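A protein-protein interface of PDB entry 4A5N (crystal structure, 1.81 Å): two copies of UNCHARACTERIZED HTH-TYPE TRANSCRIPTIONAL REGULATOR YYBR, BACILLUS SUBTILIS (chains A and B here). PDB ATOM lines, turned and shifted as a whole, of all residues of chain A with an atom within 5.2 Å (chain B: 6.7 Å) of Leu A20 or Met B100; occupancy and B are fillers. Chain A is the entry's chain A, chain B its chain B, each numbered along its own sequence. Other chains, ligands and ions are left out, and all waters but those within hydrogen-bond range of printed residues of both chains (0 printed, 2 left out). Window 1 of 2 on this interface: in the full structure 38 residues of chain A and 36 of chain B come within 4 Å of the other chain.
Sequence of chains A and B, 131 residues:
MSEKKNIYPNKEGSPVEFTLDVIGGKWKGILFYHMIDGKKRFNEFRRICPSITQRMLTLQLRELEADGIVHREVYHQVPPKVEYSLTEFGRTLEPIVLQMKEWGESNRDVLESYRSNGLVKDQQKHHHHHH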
ATOM      1  N   PRO A  15      27.478  -3.028  -5.105  1.00  0.00           N
ATOM      2  CA  PRO A  15      28.136  -3.574  -3.941  1.00  0.00           C
ATOM      3  C   PRO A  15      27.169  -4.253  -2.950  1.00  0.00           C
ATOM      4  O   PRO A  15      27.586  -5.142  -2.233  1.00  0.00           O
ATOM      5  CB  PRO A  15      28.799  -2.354  -3.298  1.00  0.00           C
ATOM      6  CG  PRO A  15      27.980  -1.198  -3.791  1.00  0.00           C
ATOM      7  CD  PRO A  15      27.646  -1.562  -5.194  1.00  0.00           C
ATOM      8  N   VAL A  16      25.902  -3.849  -2.940  1.00  0.00           N
ATOM      9  CA  VAL A  16      24.896  -4.533  -2.127  1.00  0.00           C
ATOM     10  C   VAL A  16      24.735  -5.991  -2.594  1.00  0.00           C
ATOM     11  O   VAL A  16      24.805  -6.917  -1.784  1.00  0.00           O
ATOM     12  CB  VAL A  16      23.551  -3.797  -2.165  1.00  0.00           C
ATOM     13  CG1 VAL A  16      22.522  -4.547  -1.317  1.00  0.00           C
ATOM     14  CG2 VAL A  16      23.728  -2.350  -1.684  1.00  0.00           C
ATOM     15  N   GLU A  17      24.545  -6.186  -3.903  1.00  0.00           N
ATOM     16  CA  GLU A  17      24.439  -7.529  -4.479  1.00  0.00           C
ATOM     17  C   GLU A  17      25.766  -8.320  -4.366  1.00  0.00           C
ATOM     18  O   GLU A  17      25.775  -9.566  -4.253  1.00  0.00           O
ATOM     19  CB  GLU A  17      23.966  -7.454  -5.925  1.00  0.00           C
ATOM     20  CG  GLU A  17      22.613  -6.769  -6.127  1.00  0.00           C
ATOM     21  CD  GLU A  17      21.453  -7.489  -5.432  1.00  0.00           C
ATOM     22  OE1 GLU A  17      21.643  -8.618  -4.946  1.00  0.00           O
ATOM     23  OE2 GLU A  17      20.350  -6.914  -5.373  1.00  0.00           O
ATOM     24  N   PHE A  18      26.884  -7.611  -4.332  1.00  0.00           N
ATOM     25  CA  PHE A  18      28.174  -8.268  -4.061  1.00  0.00           C
ATOM     26  C   PHE A  18      28.207  -8.952  -2.689  1.00  0.00           C
ATOM     27  O   PHE A  18      28.597 -10.112  -2.553  1.00  0.00           O
ATOM     28  CB  PHE A  18      29.292  -7.238  -4.168  1.00  0.00           C
ATOM     29  CG  PHE A  18      30.653  -7.836  -4.253  1.00  0.00           C
ATOM     30  CD1 PHE A  18      31.116  -8.336  -5.460  1.00  0.00           C
ATOM     31  CD2 PHE A  18      31.460  -7.909  -3.131  1.00  0.00           C
ATOM     32  CE1 PHE A  18      32.387  -8.907  -5.552  1.00  0.00           C
ATOM     33  CE2 PHE A  18      32.719  -8.476  -3.203  1.00  0.00           C
ATOM     34  CZ  PHE A  18      33.188  -8.971  -4.421  1.00  0.00           C
ATOM     35  N   THR A  19      27.790  -8.214  -1.663  1.00  0.00           N
ATOM     36  CA  THR A  19      27.698  -8.733  -0.312  1.00  0.00           C
ATOM     37  C   THR A  19      26.708  -9.880  -0.194  1.00  0.00           C
ATOM     38  O   THR A  19      27.015 -10.904   0.412  1.00  0.00           O
ATOM     39  CB  THR A  19      27.315  -7.605   0.652  1.00  0.00           C
ATOM     40  OG1 THR A  19      28.291  -6.577   0.512  1.00  0.00           O
ATOM     41  CG2 THR A  19      27.287  -8.087   2.101  1.00  0.00           C
ATOM     42  N   LEU A  20      25.535  -9.715  -0.796  1.00  0.00           N
ATOM     43  CA  LEU A  20      24.522 -10.781  -0.787  1.00  0.00           C
ATOM     44  C   LEU A  20      25.020 -12.072  -1.480  1.00  0.00           C
ATOM     45  O   LEU A  20      24.643 -13.173  -1.082  1.00  0.00           O
ATOM     46  CB  LEU A  20      23.223 -10.308  -1.408  1.00  0.00           C
ATOM     47  CG  LEU A  20      22.380  -9.331  -0.577  1.00  0.00           C
ATOM     48  CD1 LEU A  20      21.195  -8.804  -1.374  1.00  0.00           C
ATOM     49  CD2 LEU A  20      21.941  -9.977   0.742  1.00  0.00           C
ATOM     50  N   ASP A  21      25.911 -11.952  -2.455  1.00  0.00           N
ATOM     51  CA  ASP A  21      26.513 -13.157  -3.068  1.00  0.00           C
ATOM     52  C   ASP A  21      27.324 -13.967  -2.071  1.00  0.00           C
ATOM     53  O   ASP A  21      27.452 -15.181  -2.221  1.00  0.00           O
ATOM     54  CB  ASP A  21      27.432 -12.807  -4.241  1.00  0.00           C
ATOM     55  CG  ASP A  21      26.677 -12.493  -5.499  1.00  0.00           C
ATOM     56  OD1 ASP A  21      25.562 -13.008  -5.671  1.00  0.00           O
ATOM     57  OD2 ASP A  21      27.188 -11.709  -6.312  1.00  0.00           O
ATOM     58  N   VAL A  22      27.892 -13.288  -1.073  1.00  0.00           N
ATOM     59  CA  VAL A  22      28.780 -13.930  -0.122  1.00  0.00           C
ATOM     60  C   VAL A  22      27.996 -14.613   0.994  1.00  0.00           C
ATOM     61  O   VAL A  22      28.312 -15.742   1.395  1.00  0.00           O
ATOM     62  CB  VAL A  22      29.775 -12.913   0.468  1.00  0.00           C
ATOM     63  CG1 VAL A  22      30.561 -13.521   1.612  1.00  0.00           C
ATOM     64  CG2 VAL A  22      30.677 -12.386  -0.651  1.00  0.00           C
ATOM     65  N   ILE A  23      26.977 -13.909   1.487  1.00  0.00           N
ATOM     66  CA  ILE A  23      26.277 -14.273   2.719  1.00  0.00           C
ATOM     67  C   ILE A  23      24.836 -14.712   2.452  1.00  0.00           C
ATOM     68  O   ILE A  23      24.121 -15.087   3.381  1.00  0.00           O
ATOM     69  CB  ILE A  23      26.307 -13.063   3.696  1.00  0.00           C
ATOM     70  CG1 ILE A  23      26.266 -13.485   5.170  1.00  0.00           C
ATOM     71  CG2 ILE A  23      25.144 -12.123   3.416  1.00  0.00           C
ATOM     72  CD1 ILE A  23      27.124 -14.672   5.550  1.00  0.00           C
ATOM     73  N   GLY A  24      24.431 -14.699   1.181  1.00  0.00           N
ATOM     74  CA  GLY A  24      23.052 -14.860   0.787  1.00  0.00           C
ATOM     75  C   GLY A  24      22.642 -16.287   0.529  1.00  0.00           C
ATOM     76  O   GLY A  24      23.432 -17.204   0.664  1.00  0.00           O
ATOM     77  N   GLY A  25      21.380 -16.462   0.163  1.00  0.00           N
ATOM     78  CA  GLY A  25      20.816 -17.786  -0.055  1.00  0.00           C
ATOM     79  C   GLY A  25      20.153 -18.295   1.217  1.00  0.00           C
ATOM     80  O   GLY A  25      19.927 -17.518   2.152  1.00  0.00           O
ATOM     81  N   ILE A  96      26.467  -7.189   9.941  1.00  0.00           N
ATOM     82  CA  ILE A  96      25.399  -7.409   8.989  1.00  0.00           C
ATOM     83  C   ILE A  96      24.558  -8.616   9.418  1.00  0.00           C
ATOM     84  O   ILE A  96      23.362  -8.521   9.410  1.00  0.00           O
ATOM     85  CB  ILE A  96      25.901  -7.581   7.519  1.00  0.00           C
ATOM     86  CG1 ILE A  96      26.383  -6.233   6.963  1.00  0.00           C
ATOM     87  CG2 ILE A  96      24.766  -8.154   6.653  1.00  0.00           C
ATOM     88  CD1 ILE A  96      27.432  -6.260   5.868  1.00  0.00           C
ATOM     89  N   LEU B  20      16.815 -12.300   4.903  1.00  0.00           N
ATOM     90  CA  LEU B  20      17.370 -12.465   3.565  1.00  0.00           C
ATOM     91  C   LEU B  20      16.285 -12.810   2.526  1.00  0.00           C
ATOM     92  O   LEU B  20      16.413 -12.461   1.351  1.00  0.00           O
ATOM     93  CB  LEU B  20      18.454 -13.514   3.584  1.00  0.00           C
ATOM     94  CG  LEU B  20      19.831 -13.124   4.077  1.00  0.00           C
ATOM     95  CD1 LEU B  20      20.682 -14.375   4.250  1.00  0.00           C
ATOM     96  CD2 LEU B  20      20.549 -12.164   3.125  1.00  0.00           C
ATOM     97  N   ILE B  23      14.904  -9.277   1.466  1.00  0.00           N
ATOM     98  CA  ILE B  23      15.806  -8.309   0.828  1.00  0.00           C
ATOM     99  C   ILE B  23      16.824  -8.966  -0.103  1.00  0.00           C
ATOM    100  O   ILE B  23      17.583  -8.289  -0.791  1.00  0.00           O
ATOM    101  CB  ILE B  23      16.492  -7.424   1.908  1.00  0.00           C
ATOM    102  CG1 ILE B  23      16.892  -6.051   1.354  1.00  0.00           C
ATOM    103  CG2 ILE B  23      17.681  -8.128   2.549  1.00  0.00           C
ATOM    104  CD1 ILE B  23      15.810  -5.310   0.586  1.00  0.00           C
ATOM    105  N   GLY B  24      16.788 -10.295  -0.147  1.00  0.00           N
ATOM    106  CA  GLY B  24      17.781 -11.061  -0.865  1.00  0.00           C
ATOM    107  C   GLY B  24      17.370 -11.401  -2.263  1.00  0.00           C
ATOM    108  O   GLY B  24      16.303 -11.029  -2.733  1.00  0.00           O
ATOM    109  N   GLY B  25      18.261 -12.098  -2.944  1.00  0.00           N
ATOM    110  CA  GLY B  25      18.063 -12.429  -4.351  1.00  0.00           C
ATOM    111  C   GLY B  25      18.854 -11.434  -5.189  1.00  0.00           C
ATOM    112  O   GLY B  25      19.571 -10.601  -4.646  1.00  0.00           O
ATOM    113  N   LYS B  26      18.753 -11.517  -6.508  1.00  0.00           N
ATOM    114  CA  LYS B  26      19.637 -10.727  -7.354  1.00  0.00           C
ATOM    115  C   LYS B  26      19.331  -9.214  -7.499  1.00  0.00           C
ATOM    116  O   LYS B  26      20.226  -8.428  -7.837  1.00  0.00           O
ATOM    117  CB  LYS B  26      19.748 -11.396  -8.736  1.00  0.00           C
ATOM    118  CG  LYS B  26      20.651 -10.631  -9.670  1.00  0.00           C
ATOM    119  CD  LYS B  26      21.143 -11.484 -10.833  1.00  0.00           C
ATOM    120  CE  LYS B  26      22.368 -10.847 -11.454  1.00  0.00           C
ATOM    121  NZ  LYS B  26      23.179 -11.884 -12.153  1.00  0.00           N
ATOM    122  N   TRP B  27      18.102  -8.797  -7.190  1.00  0.00           N
ATOM    123  CA  TRP B  27      17.617  -7.496  -7.595  1.00  0.00           C
ATOM    124  C   TRP B  27      17.099  -6.632  -6.482  1.00  0.00           C
ATOM    125  O   TRP B  27      17.145  -5.429  -6.581  1.00  0.00           O
ATOM    126  CB  TRP B  27      16.484  -7.681  -8.581  1.00  0.00           C
ATOM    127  CG  TRP B  27      16.789  -8.607  -9.730  1.00  0.00           C
ATOM    128  CD1 TRP B  27      16.310  -9.886  -9.932  1.00  0.00           C
ATOM    129  CD2 TRP B  27      17.652  -8.329 -10.870  1.00  0.00           C
ATOM    130  NE1 TRP B  27      16.798 -10.413 -11.114  1.00  0.00           N
ATOM    131  CE2 TRP B  27      17.613  -9.518 -11.720  1.00  0.00           C
ATOM    132  CE3 TRP B  27      18.424  -7.248 -11.263  1.00  0.00           C
ATOM    133  CZ2 TRP B  27      18.333  -9.600 -12.889  1.00  0.00           C
ATOM    134  CZ3 TRP B  27      19.134  -7.336 -12.456  1.00  0.00           C
ATOM    135  CH2 TRP B  27      19.094  -8.488 -13.246  1.00  0.00           C
ATOM    136  N   LYS B  28      16.556  -7.214  -5.440  1.00  0.00           N
ATOM    137  CA  LYS B  28      15.828  -6.367  -4.474  1.00  0.00           C
ATOM    138  C   LYS B  28      16.731  -5.361  -3.783  1.00  0.00           C
ATOM    139  O   LYS B  28      16.301  -4.249  -3.462  1.00  0.00           O
ATOM    140  CB  LYS B  28      15.075  -7.232  -3.463  1.00  0.00           C
ATOM    141  CG  LYS B  28      13.775  -7.837  -3.979  1.00  0.00           C
ATOM    142  CD  LYS B  28      13.248  -8.896  -3.041  1.00  0.00           C
ATOM    143  CE  LYS B  28      12.139  -9.705  -3.648  1.00  0.00           C
ATOM    144  NZ  LYS B  28      11.590 -10.611  -2.623  1.00  0.00           N
ATOM    145  N   GLY B  29      17.957  -5.758  -3.467  1.00  0.00           N
ATOM    146  CA  GLY B  29      18.916  -4.854  -2.822  1.00  0.00           C
ATOM    147  C   GLY B  29      19.186  -3.585  -3.610  1.00  0.00           C
ATOM    148  O   GLY B  29      19.268  -2.485  -3.045  1.00  0.00           O
ATOM    149  N   ILE B  30      19.352  -3.753  -4.926  1.00  0.00           N
ATOM    150  CA  ILE B  30      19.605  -2.660  -5.843  1.00  0.00           C
ATOM    151  C   ILE B  30      18.385  -1.762  -5.896  1.00  0.00           C
ATOM    152  O   ILE B  30      18.516  -0.545  -5.769  1.00  0.00           O
ATOM    153  CB  ILE B  30      19.874  -3.176  -7.288  1.00  0.00           C
ATOM    154  CG1 ILE B  30      21.123  -4.042  -7.356  1.00  0.00           C
ATOM    155  CG2 ILE B  30      20.052  -2.025  -8.291  1.00  0.00           C
ATOM    156  CD1 ILE B  30      21.264  -4.784  -8.673  1.00  0.00           C
ATOM    157  N   LEU B  93      14.868  -1.379   7.174  1.00  0.00           N
ATOM    158  CA  LEU B  93      15.947  -2.168   6.583  1.00  0.00           C
ATOM    159  C   LEU B  93      17.060  -1.330   6.004  1.00  0.00           C
ATOM    160  O   LEU B  93      18.086  -1.871   5.612  1.00  0.00           O
ATOM    161  CB  LEU B  93      15.432  -3.043   5.412  1.00  0.00           C
ATOM    162  CG  LEU B  93      14.695  -4.331   5.670  1.00  0.00           C
ATOM    163  CD1 LEU B  93      13.935  -4.774   4.425  1.00  0.00           C
ATOM    164  CD2 LEU B  93      15.587  -5.472   6.137  1.00  0.00           C
ATOM    165  N   PRO B  95      19.501   0.624   7.359  1.00  0.00           N
ATOM    166  CA  PRO B  95      20.836   0.460   7.953  1.00  0.00           C
ATOM    167  C   PRO B  95      21.548  -0.793   7.514  1.00  0.00           C
ATOM    168  O   PRO B  95      22.746  -0.751   7.193  1.00  0.00           O
ATOM    169  CB  PRO B  95      20.540   0.456   9.477  1.00  0.00           C
ATOM    170  CG  PRO B  95      19.326   1.334   9.579  1.00  0.00           C
ATOM    171  CD  PRO B  95      18.491   1.042   8.371  1.00  0.00           C
ATOM    172  N   ILE B  96      20.800  -1.879   7.426  1.00  0.00           N
ATOM    173  CA  ILE B  96      21.346  -3.145   6.967  1.00  0.00           C
ATOM    174  C   ILE B  96      21.773  -3.003   5.485  1.00  0.00           C
ATOM    175  O   ILE B  96      22.882  -3.372   5.139  1.00  0.00           O
ATOM    176  CB  ILE B  96      20.332  -4.296   7.106  1.00  0.00           C
ATOM    177  CG1 ILE B  96      20.237  -4.758   8.580  1.00  0.00           C
ATOM    178  CG2 ILE B  96      20.710  -5.437   6.135  1.00  0.00           C
ATOM    179  CD1 ILE B  96      19.008  -5.582   8.934  1.00  0.00           C
ATOM    180  N   VAL B  97      20.900  -2.427   4.651  1.00  0.00           N
ATOM    181  CA  VAL B  97      21.246  -2.232   3.212  1.00  0.00           C
ATOM    182  C   VAL B  97      22.466  -1.329   3.036  1.00  0.00           C
ATOM    183  O   VAL B  97      23.368  -1.661   2.273  1.00  0.00           O
ATOM    184  CB  VAL B  97      20.045  -1.787   2.362  1.00  0.00           C
ATOM    185  CG1 VAL B  97      20.490  -1.394   0.960  1.00  0.00           C
ATOM    186  CG2 VAL B  97      19.054  -2.912   2.293  1.00  0.00           C
ATOM    187  N   LEU B  98      22.554  -0.235   3.796  1.00  0.00           N
ATOM    188  CA  LEU B  98      23.726   0.617   3.706  1.00  0.00           C
ATOM    189  C   LEU B  98      25.024  -0.110   4.171  1.00  0.00           C
ATOM    190  O   LEU B  98      26.048   0.028   3.525  1.00  0.00           O
ATOM    191  CB  LEU B  98      23.509   1.962   4.408  1.00  0.00           C
ATOM    192  CG  LEU B  98      22.518   2.939   3.757  1.00  0.00           C
ATOM    193  CD1 LEU B  98      22.502   4.235   4.565  1.00  0.00           C
ATOM    194  CD2 LEU B  98      22.832   3.239   2.297  1.00  0.00           C
ATOM    195  N   GLN B  99      24.953  -0.947   5.209  1.00  0.00           N
ATOM    196  CA  GLN B  99      26.089  -1.758   5.601  1.00  0.00           C
ATOM    197  C   GLN B  99      26.567  -2.707   4.530  1.00  0.00           C
ATOM    198  O   GLN B  99      27.806  -2.842   4.347  1.00  0.00           O
ATOM    199  CB  GLN B  99      25.799  -2.524   6.860  1.00  0.00           C
ATOM    200  CG  GLN B  99      25.858  -1.612   8.065  1.00  0.00           C
ATOM    201  CD  GLN B  99      25.433  -2.338   9.298  1.00  0.00           C
ATOM    202  OE1 GLN B  99      26.178  -3.160   9.851  1.00  0.00           O
ATOM    203  NE2 GLN B  99      24.195  -2.049   9.743  1.00  0.00           N
ATOM    204  N   MET B 100      25.621  -3.318   3.823  1.00  0.00           N
ATOM    205  CA  MET B 100      25.961  -4.194   2.702  1.00  0.00           C
ATOM    206  C   MET B 100      26.694  -3.400   1.605  1.00  0.00           C
ATOM    207  O   MET B 100      27.700  -3.870   1.049  1.00  0.00           O
ATOM    208  CB  MET B 100      24.726  -4.890   2.148  1.00  0.00           C
ATOM    209  CG  MET B 100      24.092  -5.858   3.150  1.00  0.00           C
ATOM    210  SD  MET B 100      22.756  -6.876   2.555  1.00  0.00           S
ATOM    211  CE  MET B 100      21.580  -5.798   1.796  1.00  0.00           C
ATOM    212  N   LYS B 101      26.191  -2.216   1.285  1.00  0.00           N
ATOM    213  CA  LYS B 101      26.852  -1.354   0.309  1.00  0.00           C
ATOM    214  C   LYS B 101      28.323  -1.143   0.730  1.00  0.00           C
ATOM    215  O   LYS B 101      29.264  -1.395  -0.052  1.00  0.00           O
ATOM    216  CB  LYS B 101      26.155   0.035   0.186  1.00  0.00           C
ATOM    217  CG  LYS B 101      26.897   0.953  -0.785  1.00  0.00           C
ATOM    218  CD  LYS B 101      26.370   2.378  -0.839  1.00  0.00           C
ATOM    219  CE  LYS B 101      27.184   3.282  -1.770  1.00  0.00           C
ATOM    220  NZ  LYS B 101      28.539   3.673  -1.264  1.00  0.00           N
ATOM    221  N   GLU B 102      28.505  -0.655   1.955  1.00  0.00           N
ATOM    222  CA  GLU B 102      29.838  -0.328   2.470  1.00  0.00           C
ATOM    223  C   GLU B 102      30.764  -1.537   2.507  1.00  0.00           C
ATOM    224  O   GLU B 102      31.905  -1.471   2.010  1.00  0.00           O
ATOM    225  CB  GLU B 102      29.745   0.306   3.859  1.00  0.00           C
ATOM    226  CG  GLU B 102      29.179   1.723   3.845  1.00  0.00           C
ATOM    227  CD  GLU B 102      29.961   2.659   2.916  1.00  0.00           C
ATOM    228  OE1 GLU B 102      31.204   2.635   2.979  1.00  0.00           O
ATOM    229  OE2 GLU B 102      29.349   3.398   2.107  1.00  0.00           O
ATOM    230  N   TRP B 103      30.258  -2.661   3.019  1.00  0.00           N
ATOM    231  CA  TRP B 103      31.092  -3.856   3.181  1.00  0.00           C
ATOM    232  C   TRP B 103      31.493  -4.338   1.813  1.00  0.00           C
ATOM    233  O   TRP B 103      32.652  -4.683   1.583  1.00  0.00           O
ATOM    234  CB  TRP B 103      30.353  -4.956   3.925  1.00  0.00           C
ATOM    235  CG  TRP B 103      31.201  -6.143   4.268  1.00  0.00           C
ATOM    236  CD1 TRP B 103      31.881  -6.369   5.449  1.00  0.00           C
ATOM    237  CD2 TRP B 103      31.504  -7.318   3.414  1.00  0.00           C
ATOM    238  NE1 TRP B 103      32.563  -7.550   5.397  1.00  0.00           N
ATOM    239  CE2 TRP B 103      32.391  -8.162   4.193  1.00  0.00           C
ATOM    240  CE3 TRP B 103      31.135  -7.725   2.126  1.00  0.00           C
ATOM    241  CZ2 TRP B 103      32.885  -9.377   3.695  1.00  0.00           C
ATOM    242  CZ3 TRP B 103      31.641  -8.924   1.634  1.00  0.00           C
ATOM    243  CH2 TRP B 103      32.497  -9.738   2.400  1.00  0.00           C
ATOM    244  N   GLY B 104      30.552  -4.274   0.881  1.00  0.00           N
ATOM    245  CA  GLY B 104      30.812  -4.711  -0.493  1.00  0.00           C
ATOM    246  C   GLY B 104      31.820  -3.832  -1.200  1.00  0.00           C
ATOM    247  O   GLY B 104      32.670  -4.324  -1.990  1.00  0.00           O
ATOM    248  N   GLU B 105      31.718  -2.524  -0.976  1.00  0.00           N
ATOM    249  CA  GLU B 105      32.688  -1.571  -1.545  1.00  0.00           C
ATOM    250  C   GLU B 105      34.091  -1.768  -0.987  1.00  0.00           C
ATOM    251  O   GLU B 105      35.053  -1.850  -1.732  1.00  0.00           O
ATOM    252  CB  GLU B 105      32.268  -0.119  -1.269  1.00  0.00           C
ATOM    253  CG  GLU B 105      31.374   0.432  -2.338  1.00  0.00           C
ATOM    254  CD  GLU B 105      30.751   1.762  -1.967  1.00  0.00           C
ATOM    255  OE1 GLU B 105      30.827   2.165  -0.779  1.00  0.00           O
ATOM    256  OE2 GLU B 105      30.148   2.372  -2.862  1.00  0.00           O
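Of the 21 printed residues of chain B, 14 touch a printed residue of chain A.
Printed residues of chain B that touch a printed residue of chain A: Leu B20, Ile B23, Gly B25, Lys B26, Trp B27, Lys B28, Gly B29, Ile B30, Gln B99, Met B100, Lys B101, Trp B103, Gly B104 and Glu B105.
Along chain B the printed residues that touch a printed residue of chain A span positions 20 to 105.
Hydrophobic or aromatic side chains of chain A within 4 Å of the printed part of chain B: Pro A15, Val A16, Phe A18, Leu A20 and Ile A96.
Among the printed residues, 24 pairs touch across the chains.
Among the printed residues, no Asp or Glu carboxylate lies within 4 Å of a Lys or Arg side-chain nitrogen of the other chain.
The backbone carbonyl oxygen (O) of Pro A15 is in hydrogen-bond range of the side-chain hydroxyl (OG1) of Thr A19 (3.2 Å).
The side-chain amide nitrogen (NE2) of Gln B99 sits at hydrogen-bond distance from the backbone carbonyl oxygen (O) of Pro B95 (3.2 Å).
OE2 of Glu B102 is in salt-bridge range of NZ of Lys B101.
The side-chain amino group (NZ) of Lys B101 lies within salt-bridge range of the side-chain carboxylate (OE2) of Glu B105, 2.6 Å away.
Leu A20 touches its own counterpart, Leu B20.
Leu A20 touches Ile B23, and with the chains exchanged Ile A23 touches Leu B20.
Gly A25 touches Leu B20, but with the chains exchanged Leu A20 does not touch Gly B25 (4.1 Å).
5 positions are printed for both chains.
Of the 24 pairs that touch across the chains among the printed residues, 3 have their exchanged pair printed and touching as well.
The backbone NH of Trp B27 lies close to the side-chain carboxylate of Glu A17 (3.4 Å).
The side-chain carboxylate (OE2) of Glu A17 sits at hydrogen-bond distance from the backbone NH (N) of Gly B29, at 3.3 Å.
The backbone NH (N) of Ile B30 lies within hydrogen-bond range of the side-chain carboxylate (OE2) of Glu A17, 3.3 Å away.
The side-chain hydroxyl (OG1) of Thr A19 sits at hydrogen-bond distance from the backbone carbonyl oxygen (O) of Met B100.
N of Gly B104 sits at hydrogen-bond distance from OG1 of Thr A19, at 3.2 Å.
O of Gly B25 sits close to OE1 of Glu A17, at 2.9 Å.
OE2 of Glu A17 sits close to O of Lys B26 (2.9 Å).
Leu A20 touches just these residues of chain B: Leu B20, Ile B23 and Met B100.
Of the printed residues of chain A, Met B100 touches Pro A15, Val A16, Thr A19 and Leu A20.
Printed residues of chain B within 4 Å of Gly A25: Leu B20.
Of the printed residues of chain A, Gln B99 touches Ile A96.
Ile B96 touches none of the printed residues of chain A.
The nearest printed residue of chain A that does not touch Met B100 is Ile A96 (4.01 Å).
The nearest printed residue of chain B that does not touch Thr A19 is Lys B101 (4.9 Å).
Among the printed residues, pairs that only touch across the chains: Pro A15 with Lys B101 (3.4 Å), Thr A19 with Trp B103 (3.5 Å), Val A16 with Met B100 (3.5 Å), Leu A20 with Leu B20 (3.5 Å), Pro A15 with Met B100 (3.5 Å), Ile A23 with Leu B20 (3.6 Å), Leu A20 with Met B100 (3.7 Å), Pro A15 with Gly B104 (3.7 Å), Leu A20 with Ile B23 (3.7 Å), Pro A15 with Glu B105 (3.7 Å), Ile A96 with Trp B103 (3.7 Å), Ile A96 with Gln B99 (3.8 Å), Glu A17 with Lys B28 (3.8 Å), Val A16 with Lys B101 (3.8 Å), Gly A25 with Leu B20 (3.9 Å), Val A16 with Gly B29 (3.9 Å) and Phe A18 with Gly B104 (3.95 Å).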
